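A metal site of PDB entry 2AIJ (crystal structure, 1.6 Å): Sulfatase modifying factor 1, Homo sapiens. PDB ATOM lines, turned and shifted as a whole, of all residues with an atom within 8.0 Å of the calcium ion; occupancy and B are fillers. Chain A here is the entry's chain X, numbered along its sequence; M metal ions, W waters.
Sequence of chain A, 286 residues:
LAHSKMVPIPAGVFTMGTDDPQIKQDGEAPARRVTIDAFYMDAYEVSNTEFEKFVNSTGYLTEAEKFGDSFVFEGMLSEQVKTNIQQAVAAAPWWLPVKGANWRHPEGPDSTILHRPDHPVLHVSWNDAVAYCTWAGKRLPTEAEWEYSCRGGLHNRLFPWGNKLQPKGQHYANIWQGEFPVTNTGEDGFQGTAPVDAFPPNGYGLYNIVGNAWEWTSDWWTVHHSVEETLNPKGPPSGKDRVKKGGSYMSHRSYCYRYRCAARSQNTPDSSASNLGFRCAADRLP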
ATOM      1  N   TYR A  44       9.365  10.200  18.326  1.00  0.00           N
ATOM      2  CA  TYR A  44      10.636   9.498  18.240  1.00  0.00           C
ATOM      3  C   TYR A  44      11.689  10.228  19.039  1.00  0.00           C
ATOM      4  O   TYR A  44      11.661  11.453  19.165  1.00  0.00           O
ATOM      5  CB  TYR A  44      11.084   9.490  16.782  1.00  0.00           C
ATOM      6  CG  TYR A  44      10.035   9.002  15.810  1.00  0.00           C
ATOM      7  CD1 TYR A  44       9.652   7.686  15.783  1.00  0.00           C
ATOM      8  CD2 TYR A  44       9.410   9.895  14.927  1.00  0.00           C
ATOM      9  CE1 TYR A  44       8.671   7.224  14.919  1.00  0.00           C
ATOM     10  CE2 TYR A  44       8.457   9.431  14.046  1.00  0.00           C
ATOM     11  CZ  TYR A  44       8.102   8.095  14.034  1.00  0.00           C
ATOM     12  OH  TYR A  44       7.139   7.603  13.156  1.00  0.00           O
ATOM     13  N   GLU A  45      12.682   9.484  19.515  1.00  0.00           N
ATOM     14  CA  GLU A  45      13.909  10.130  19.959  1.00  0.00           C
ATOM     15  C   GLU A  45      14.450  10.981  18.802  1.00  0.00           C
ATOM     16  O   GLU A  45      14.254  10.632  17.646  1.00  0.00           O
ATOM     17  CB  GLU A  45      14.945   9.066  20.271  1.00  0.00           C
ATOM     18  CG  GLU A  45      14.623   8.210  21.482  1.00  0.00           C
ATOM     19  CD  GLU A  45      15.203   6.801  21.450  1.00  0.00           C
ATOM     20  OE1 GLU A  45      15.309   6.194  20.391  1.00  0.00           O
ATOM     21  OE2 GLU A  45      15.437   6.238  22.553  1.00  0.00           O
ATOM     22  N   PRO A 120      18.968   7.167  17.116  1.00  0.00           N
ATOM     23  CA  PRO A 120      18.972   8.331  18.001  1.00  0.00           C
ATOM     24  C   PRO A 120      20.318   8.978  18.081  1.00  0.00           C
ATOM     25  O   PRO A 120      21.328   8.300  18.114  1.00  0.00           O
ATOM     26  CB  PRO A 120      18.651   7.724  19.367  1.00  0.00           C
ATOM     27  CG  PRO A 120      18.999   6.266  19.222  1.00  0.00           C
ATOM     28  CD  PRO A 120      18.654   5.925  17.822  1.00  0.00           C
ATOM     29  N   TRP A 146       7.085  13.324  30.891  1.00  0.00           N
ATOM     30  CA  TRP A 146       7.763  12.175  30.278  1.00  0.00           C
ATOM     31  C   TRP A 146       7.151  10.859  30.761  1.00  0.00           C
ATOM     32  O   TRP A 146       6.798   9.954  29.963  1.00  0.00           O
ATOM     33  CB  TRP A 146       9.257  12.223  30.578  1.00  0.00           C
ATOM     34  CG  TRP A 146      10.021  11.239  29.752  1.00  0.00           C
ATOM     35  CD1 TRP A 146      10.702  11.477  28.603  1.00  0.00           C
ATOM     36  CD2 TRP A 146      10.138   9.838  30.005  1.00  0.00           C
ATOM     37  NE1 TRP A 146      11.244  10.296  28.131  1.00  0.00           N
ATOM     38  CE2 TRP A 146      10.932   9.279  28.981  1.00  0.00           C
ATOM     39  CE3 TRP A 146       9.692   8.994  31.029  1.00  0.00           C
ATOM     40  CZ2 TRP A 146      11.215   7.908  28.932  1.00  0.00           C
ATOM     41  CZ3 TRP A 146       9.978   7.642  30.959  1.00  0.00           C
ATOM     42  CH2 TRP A 146      10.753   7.122  29.929  1.00  0.00           C
ATOM     43  N   ASN A 174      14.333  -2.039  22.869  1.00  0.00           N
ATOM     44  CA  ASN A 174      15.710  -2.406  22.650  1.00  0.00           C
ATOM     45  C   ASN A 174      16.474  -2.233  23.959  1.00  0.00           C
ATOM     46  O   ASN A 174      16.848  -1.155  24.334  1.00  0.00           O
ATOM     47  CB  ASN A 174      16.306  -1.539  21.564  1.00  0.00           C
ATOM     48  CG  ASN A 174      17.747  -1.846  21.322  1.00  0.00           C
ATOM     49  OD1 ASN A 174      18.203  -2.917  21.708  1.00  0.00           O
ATOM     50  ND2 ASN A 174      18.488  -0.898  20.746  1.00  0.00           N
ATOM     51  N   TYR A 207       7.503   5.892  20.281  1.00  0.00           N
ATOM     52  CA  TYR A 207       8.442   4.816  19.969  1.00  0.00           C
ATOM     53  C   TYR A 207       9.664   4.921  20.882  1.00  0.00           C
ATOM     54  O   TYR A 207      10.168   6.035  21.126  1.00  0.00           O
ATOM     55  CB  TYR A 207       8.882   4.907  18.493  1.00  0.00           C
ATOM     56  CG  TYR A 207       7.760   4.642  17.528  1.00  0.00           C
ATOM     57  CD1 TYR A 207       6.800   5.626  17.260  1.00  0.00           C
ATOM     58  CD2 TYR A 207       7.618   3.373  16.958  1.00  0.00           C
ATOM     59  CE1 TYR A 207       5.724   5.353  16.418  1.00  0.00           C
ATOM     60  CE2 TYR A 207       6.586   3.090  16.085  1.00  0.00           C
ATOM     61  CZ  TYR A 207       5.637   4.103  15.816  1.00  0.00           C
ATOM     62  OH  TYR A 207       4.588   3.796  14.957  1.00  0.00           O
ATOM     63  N   ASN A 208      10.120   3.762  21.380  1.00  0.00           N
ATOM     64  CA  ASN A 208      11.383   3.623  22.129  1.00  0.00           C
ATOM     65  C   ASN A 208      11.452   4.538  23.316  1.00  0.00           C
ATOM     66  O   ASN A 208      12.519   5.006  23.711  1.00  0.00           O
ATOM     67  CB  ASN A 208      12.553   3.807  21.200  1.00  0.00           C
ATOM     68  CG  ASN A 208      12.560   2.784  20.108  1.00  0.00           C
ATOM     69  OD1 ASN A 208      12.745   1.585  20.399  1.00  0.00           O
ATOM     70  ND2 ASN A 208      12.328   3.207  18.872  1.00  0.00           N
ATOM     71  N   ILE A 209      10.308   4.803  23.934  1.00  0.00           N
ATOM     72  CA  ILE A 209      10.275   5.589  25.153  1.00  0.00           C
ATOM     73  C   ILE A 209      10.977   4.884  26.337  1.00  0.00           C
ATOM     74  O   ILE A 209      11.641   5.549  27.138  1.00  0.00           O
ATOM     75  CB  ILE A 209       8.830   6.046  25.500  1.00  0.00           C
ATOM     76  CG1 ILE A 209       8.846   7.153  26.546  1.00  0.00           C
ATOM     77  CG2 ILE A 209       7.968   4.894  25.895  1.00  0.00           C
ATOM     78  CD1 ILE A 209       9.212   8.463  26.003  1.00  0.00           C
ATOM     79  N   VAL A 210      10.875   3.566  26.444  1.00  0.00           N
ATOM     80  CA  VAL A 210      11.855   2.786  27.230  1.00  0.00           C
ATOM     81  C   VAL A 210      12.838   2.107  26.287  1.00  0.00           C
ATOM     82  O   VAL A 210      12.490   1.691  25.163  1.00  0.00           O
ATOM     83  CB  VAL A 210      11.237   1.803  28.228  1.00  0.00           C
ATOM     84  CG1 VAL A 210      10.383   2.555  29.226  1.00  0.00           C
ATOM     85  CG2 VAL A 210      10.443   0.683  27.576  1.00  0.00           C
ATOM     86  N   GLY A 211      14.073   1.936  26.765  1.00  0.00           N
ATOM     87  CA  GLY A 211      15.124   1.399  25.920  1.00  0.00           C
ATOM     88  C   GLY A 211      15.676   2.293  24.833  1.00  0.00           C
ATOM     89  O   GLY A 211      15.271   3.438  24.692  1.00  0.00           O
ATOM     90  N   ASN A 212      16.609   1.763  24.044  1.00  0.00           N
ATOM     91  CA  ASN A 212      17.305   2.441  22.956  1.00  0.00           C
ATOM     92  C   ASN A 212      18.252   3.464  23.534  1.00  0.00           C
ATOM     93  O   ASN A 212      19.329   3.060  23.973  1.00  0.00           O
ATOM     94  CB  ASN A 212      16.330   2.981  21.881  1.00  0.00           C
ATOM     95  CG  ASN A 212      16.880   2.819  20.471  1.00  0.00           C
ATOM     96  OD1 ASN A 212      17.630   1.852  20.201  1.00  0.00           O
ATOM     97  ND2 ASN A 212      16.492   3.702  19.537  1.00  0.00           N
ATOM     98  N   ALA A 213      17.895   4.744  23.567  1.00  0.00           N
ATOM     99  CA  ALA A 213      18.701   5.775  24.237  1.00  0.00           C
ATOM    100  C   ALA A 213      17.954   6.206  25.506  1.00  0.00           C
ATOM    101  O   ALA A 213      16.707   6.311  25.501  1.00  0.00           O
ATOM    102  CB  ALA A 213      18.905   6.959  23.340  1.00  0.00           C
ATOM    103  N   TRP A 214      18.682   6.430  26.608  1.00  0.00           N
ATOM    104  CA  TRP A 214      18.170   7.190  27.747  1.00  0.00           C
ATOM    105  C   TRP A 214      17.695   8.549  27.243  1.00  0.00           C
ATOM    106  O   TRP A 214      18.183   9.033  26.219  1.00  0.00           O
ATOM    107  CB  TRP A 214      19.308   7.474  28.750  1.00  0.00           C
ATOM    108  CG  TRP A 214      19.547   6.406  29.746  1.00  0.00           C
ATOM    109  CD1 TRP A 214      20.509   5.448  29.675  1.00  0.00           C
ATOM    110  CD2 TRP A 214      18.876   6.225  30.986  1.00  0.00           C
ATOM    111  NE1 TRP A 214      20.467   4.650  30.806  1.00  0.00           N
ATOM    112  CE2 TRP A 214      19.460   5.092  31.620  1.00  0.00           C
ATOM    113  CE3 TRP A 214      17.839   6.880  31.624  1.00  0.00           C
ATOM    114  CZ2 TRP A 214      19.022   4.617  32.858  1.00  0.00           C
ATOM    115  CZ3 TRP A 214      17.388   6.399  32.865  1.00  0.00           C
ATOM    116  CH2 TRP A 214      17.971   5.285  33.459  1.00  0.00           C
ATOM    117  N   GLU A 215      16.793   9.204  27.995  1.00  0.00           N
ATOM    118  CA  GLU A 215      16.253  10.475  27.557  1.00  0.00           C
ATOM    119  C   GLU A 215      16.299  11.562  28.627  1.00  0.00           C
ATOM    120  O   GLU A 215      15.758  11.360  29.695  1.00  0.00           O
ATOM    121  CB  GLU A 215      14.826  10.248  27.087  1.00  0.00           C
ATOM    122  CG  GLU A 215      14.836   9.243  25.974  1.00  0.00           C
ATOM    123  CD  GLU A 215      13.468   8.898  25.389  1.00  0.00           C
ATOM    124  OE1 GLU A 215      12.507   9.629  25.581  1.00  0.00           O
ATOM    125  OE2 GLU A 215      13.399   7.868  24.662  1.00  0.00           O
ATOM    126  N   LYS A 245      15.443   9.507  31.922  1.00  0.00           N
ATOM    127  CA  LYS A 245      14.435   8.466  32.053  1.00  0.00           C
ATOM    128  C   LYS A 245      14.563   7.417  30.956  1.00  0.00           C
ATOM    129  O   LYS A 245      15.087   7.689  29.882  1.00  0.00           O
ATOM    130  CB  LYS A 245      13.021   9.039  31.975  1.00  0.00           C
ATOM    131  CG  LYS A 245      12.688  10.080  33.055  1.00  0.00           C
ATOM    132  CD  LYS A 245      12.264   9.434  34.372  1.00  0.00           C
ATOM    133  CE  LYS A 245      10.791   8.975  34.423  1.00  0.00           C
ATOM    134  NZ  LYS A 245      10.503   8.575  35.854  1.00  0.00           N
ATOM    135  N   GLY A 246      14.041   6.237  31.298  1.00  0.00           N
ATOM    136  CA  GLY A 246      13.659   5.223  30.321  1.00  0.00           C
ATOM    137  C   GLY A 246      14.601   4.071  30.008  1.00  0.00           C
ATOM    138  O   GLY A 246      14.205   3.147  29.301  1.00  0.00           O
ATOM    139  N   GLY A 247      15.845   4.153  30.465  1.00  0.00           N
ATOM    140  CA  GLY A 247      16.813   3.129  30.137  1.00  0.00           C
ATOM    141  C   GLY A 247      17.235   3.164  28.685  1.00  0.00           C
ATOM    142  O   GLY A 247      16.893   4.087  27.935  1.00  0.00           O
ATOM    143  N   SER A 248      18.054   2.183  28.307  1.00  0.00           N
ATOM    144  CA  SER A 248      18.759   2.198  27.028  1.00  0.00           C
ATOM    145  C   SER A 248      18.966   0.768  26.536  1.00  0.00           C
ATOM    146  O   SER A 248      18.624  -0.220  27.198  1.00  0.00           O
ATOM    147  CB  SER A 248      20.113   2.879  27.179  1.00  0.00           C
ATOM    148  OG  SER A 248      21.090   2.023  27.791  1.00  0.00           O
ATOM    149  N   TYR A 249      19.650   0.683  25.394  1.00  0.00           N
ATOM    150  CA  TYR A 249      20.038  -0.618  24.843  1.00  0.00           C
ATOM    151  C   TYR A 249      20.970  -1.458  25.720  1.00  0.00           C
ATOM    152  O   TYR A 249      21.141  -2.681  25.492  1.00  0.00           O
ATOM    153  CB  TYR A 249      20.657  -0.406  23.461  1.00  0.00           C
ATOM    154  CG  TYR A 249      22.005   0.252  23.428  1.00  0.00           C
ATOM    155  CD1 TYR A 249      22.175   1.635  23.112  1.00  0.00           C
ATOM    156  CD2 TYR A 249      23.135  -0.514  23.619  1.00  0.00           C
ATOM    157  CE1 TYR A 249      23.457   2.199  23.052  1.00  0.00           C
ATOM    158  CE2 TYR A 249      24.400   0.048  23.583  1.00  0.00           C
ATOM    159  CZ  TYR A 249      24.554   1.384  23.280  1.00  0.00           C
ATOM    160  OH  TYR A 249      25.834   1.894  23.210  1.00  0.00           O
ATOM    161  N   ASN A 275      24.952   6.122  25.359  1.00  0.00           N
ATOM    162  CA  ASN A 275      23.628   5.533  25.571  1.00  0.00           C
ATOM    163  C   ASN A 275      22.577   6.552  25.979  1.00  0.00           C
ATOM    164  O   ASN A 275      21.512   6.176  26.484  1.00  0.00           O
ATOM    165  CB  ASN A 275      23.702   4.437  26.624  1.00  0.00           C
ATOM    166  CG  ASN A 275      23.942   4.958  28.017  1.00  0.00           C
ATOM    167  OD1 ASN A 275      24.319   6.108  28.218  1.00  0.00           O
ATOM    168  ND2 ASN A 275      23.738   4.073  29.018  1.00  0.00           N
ATOM    169  N   GLY A 277      20.360  10.088  24.914  1.00  0.00           N
ATOM    170  CA  GLY A 277      19.825  11.036  23.940  1.00  0.00           C
ATOM    171  C   GLY A 277      18.640  11.756  24.539  1.00  0.00           C
ATOM    172  O   GLY A 277      18.643  12.096  25.737  1.00  0.00           O
ATOM    173  N   PHE A 278      17.649  12.051  23.691  1.00  0.00           N
ATOM    174  CA  PHE A 278      16.512  12.837  24.137  1.00  0.00           C
ATOM    175  C   PHE A 278      15.421  12.918  23.074  1.00  0.00           C
ATOM    176  O   PHE A 278      15.668  12.581  21.914  1.00  0.00           O
ATOM    177  CB  PHE A 278      16.929  14.264  24.515  1.00  0.00           C
ATOM    178  CG  PHE A 278      17.362  15.102  23.341  1.00  0.00           C
ATOM    179  CD1 PHE A 278      16.521  16.053  22.822  1.00  0.00           C
ATOM    180  CD2 PHE A 278      18.602  14.943  22.764  1.00  0.00           C
ATOM    181  CE1 PHE A 278      16.928  16.854  21.746  1.00  0.00           C
ATOM    182  CE2 PHE A 278      18.975  15.701  21.664  1.00  0.00           C
ATOM    183  CZ  PHE A 278      18.147  16.648  21.163  1.00  0.00           C
ATOM    184  N   ARG A 279      14.256  13.392  23.514  1.00  0.00           N
ATOM    185  CA  ARG A 279      13.162  13.765  22.607  1.00  0.00           C
ATOM    186  C   ARG A 279      12.584  15.076  23.180  1.00  0.00           C
ATOM    187  O   ARG A 279      12.794  15.411  24.374  1.00  0.00           O
ATOM    188  CB  ARG A 279      12.057  12.726  22.544  1.00  0.00           C
ATOM    189  CG  ARG A 279      11.154  12.652  23.732  1.00  0.00           C
ATOM    190  CD  ARG A 279      10.121  11.531  23.541  1.00  0.00           C
ATOM    191  NE  ARG A 279      10.761  10.208  23.528  1.00  0.00           N
ATOM    192  CZ  ARG A 279      10.445   9.172  22.741  1.00  0.00           C
ATOM    193  NH1 ARG A 279       9.489   9.275  21.803  1.00  0.00           N
ATOM    194  NH2 ARG A 279      11.139   8.030  22.840  1.00  0.00           N
HETATM  195 CA    CA M   1      14.530   5.796  24.650  1.00  0.00          CA
HETATM  196  O   HOH W   1      14.374   5.521  26.955  1.00  0.00           O
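The side-chain carboxylate (OE1) of Glu 45 is in hydrogen-bond range of the side-chain amide nitrogen (ND2) of Asn 212 (2.9 Å).
The backbone carbonyl oxygen (O) of Asn 208 sits close to the guanidinium group (NH2) of Arg 279 (3.4 Å).
N of Gly 211 lies within hydrogen-bond range of O of Gly 246, at 2.8 Å.
The side-chain carboxylate (OE1) of Glu 215 lies within hydrogen-bond range of the indole nitrogen (NE1) of Trp 146, 2.9 Å away.
O of Glu 215 is in hydrogen-bond range of N of Lys 245, 2.9 Å away.
The guanidinium group of Arg 279 lies within salt-bridge range of the side-chain carboxylate of Glu 215, at 2.8 Å.
Merely in contact with the calcium ion: Ile 209 (3.8 Å).
Of the 23 residues printed, 6 come within 4 Å of the calcium ion.
The calcium ion is bound by water W1, the side-chain carboxylate of Glu 45, the backbone carbonyl oxygen of Asn 208, the side-chain carboxylate of Glu 215, the backbone carbonyl oxygen of Ala 213 and the backbone carbonyl oxygen of Gly 211.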
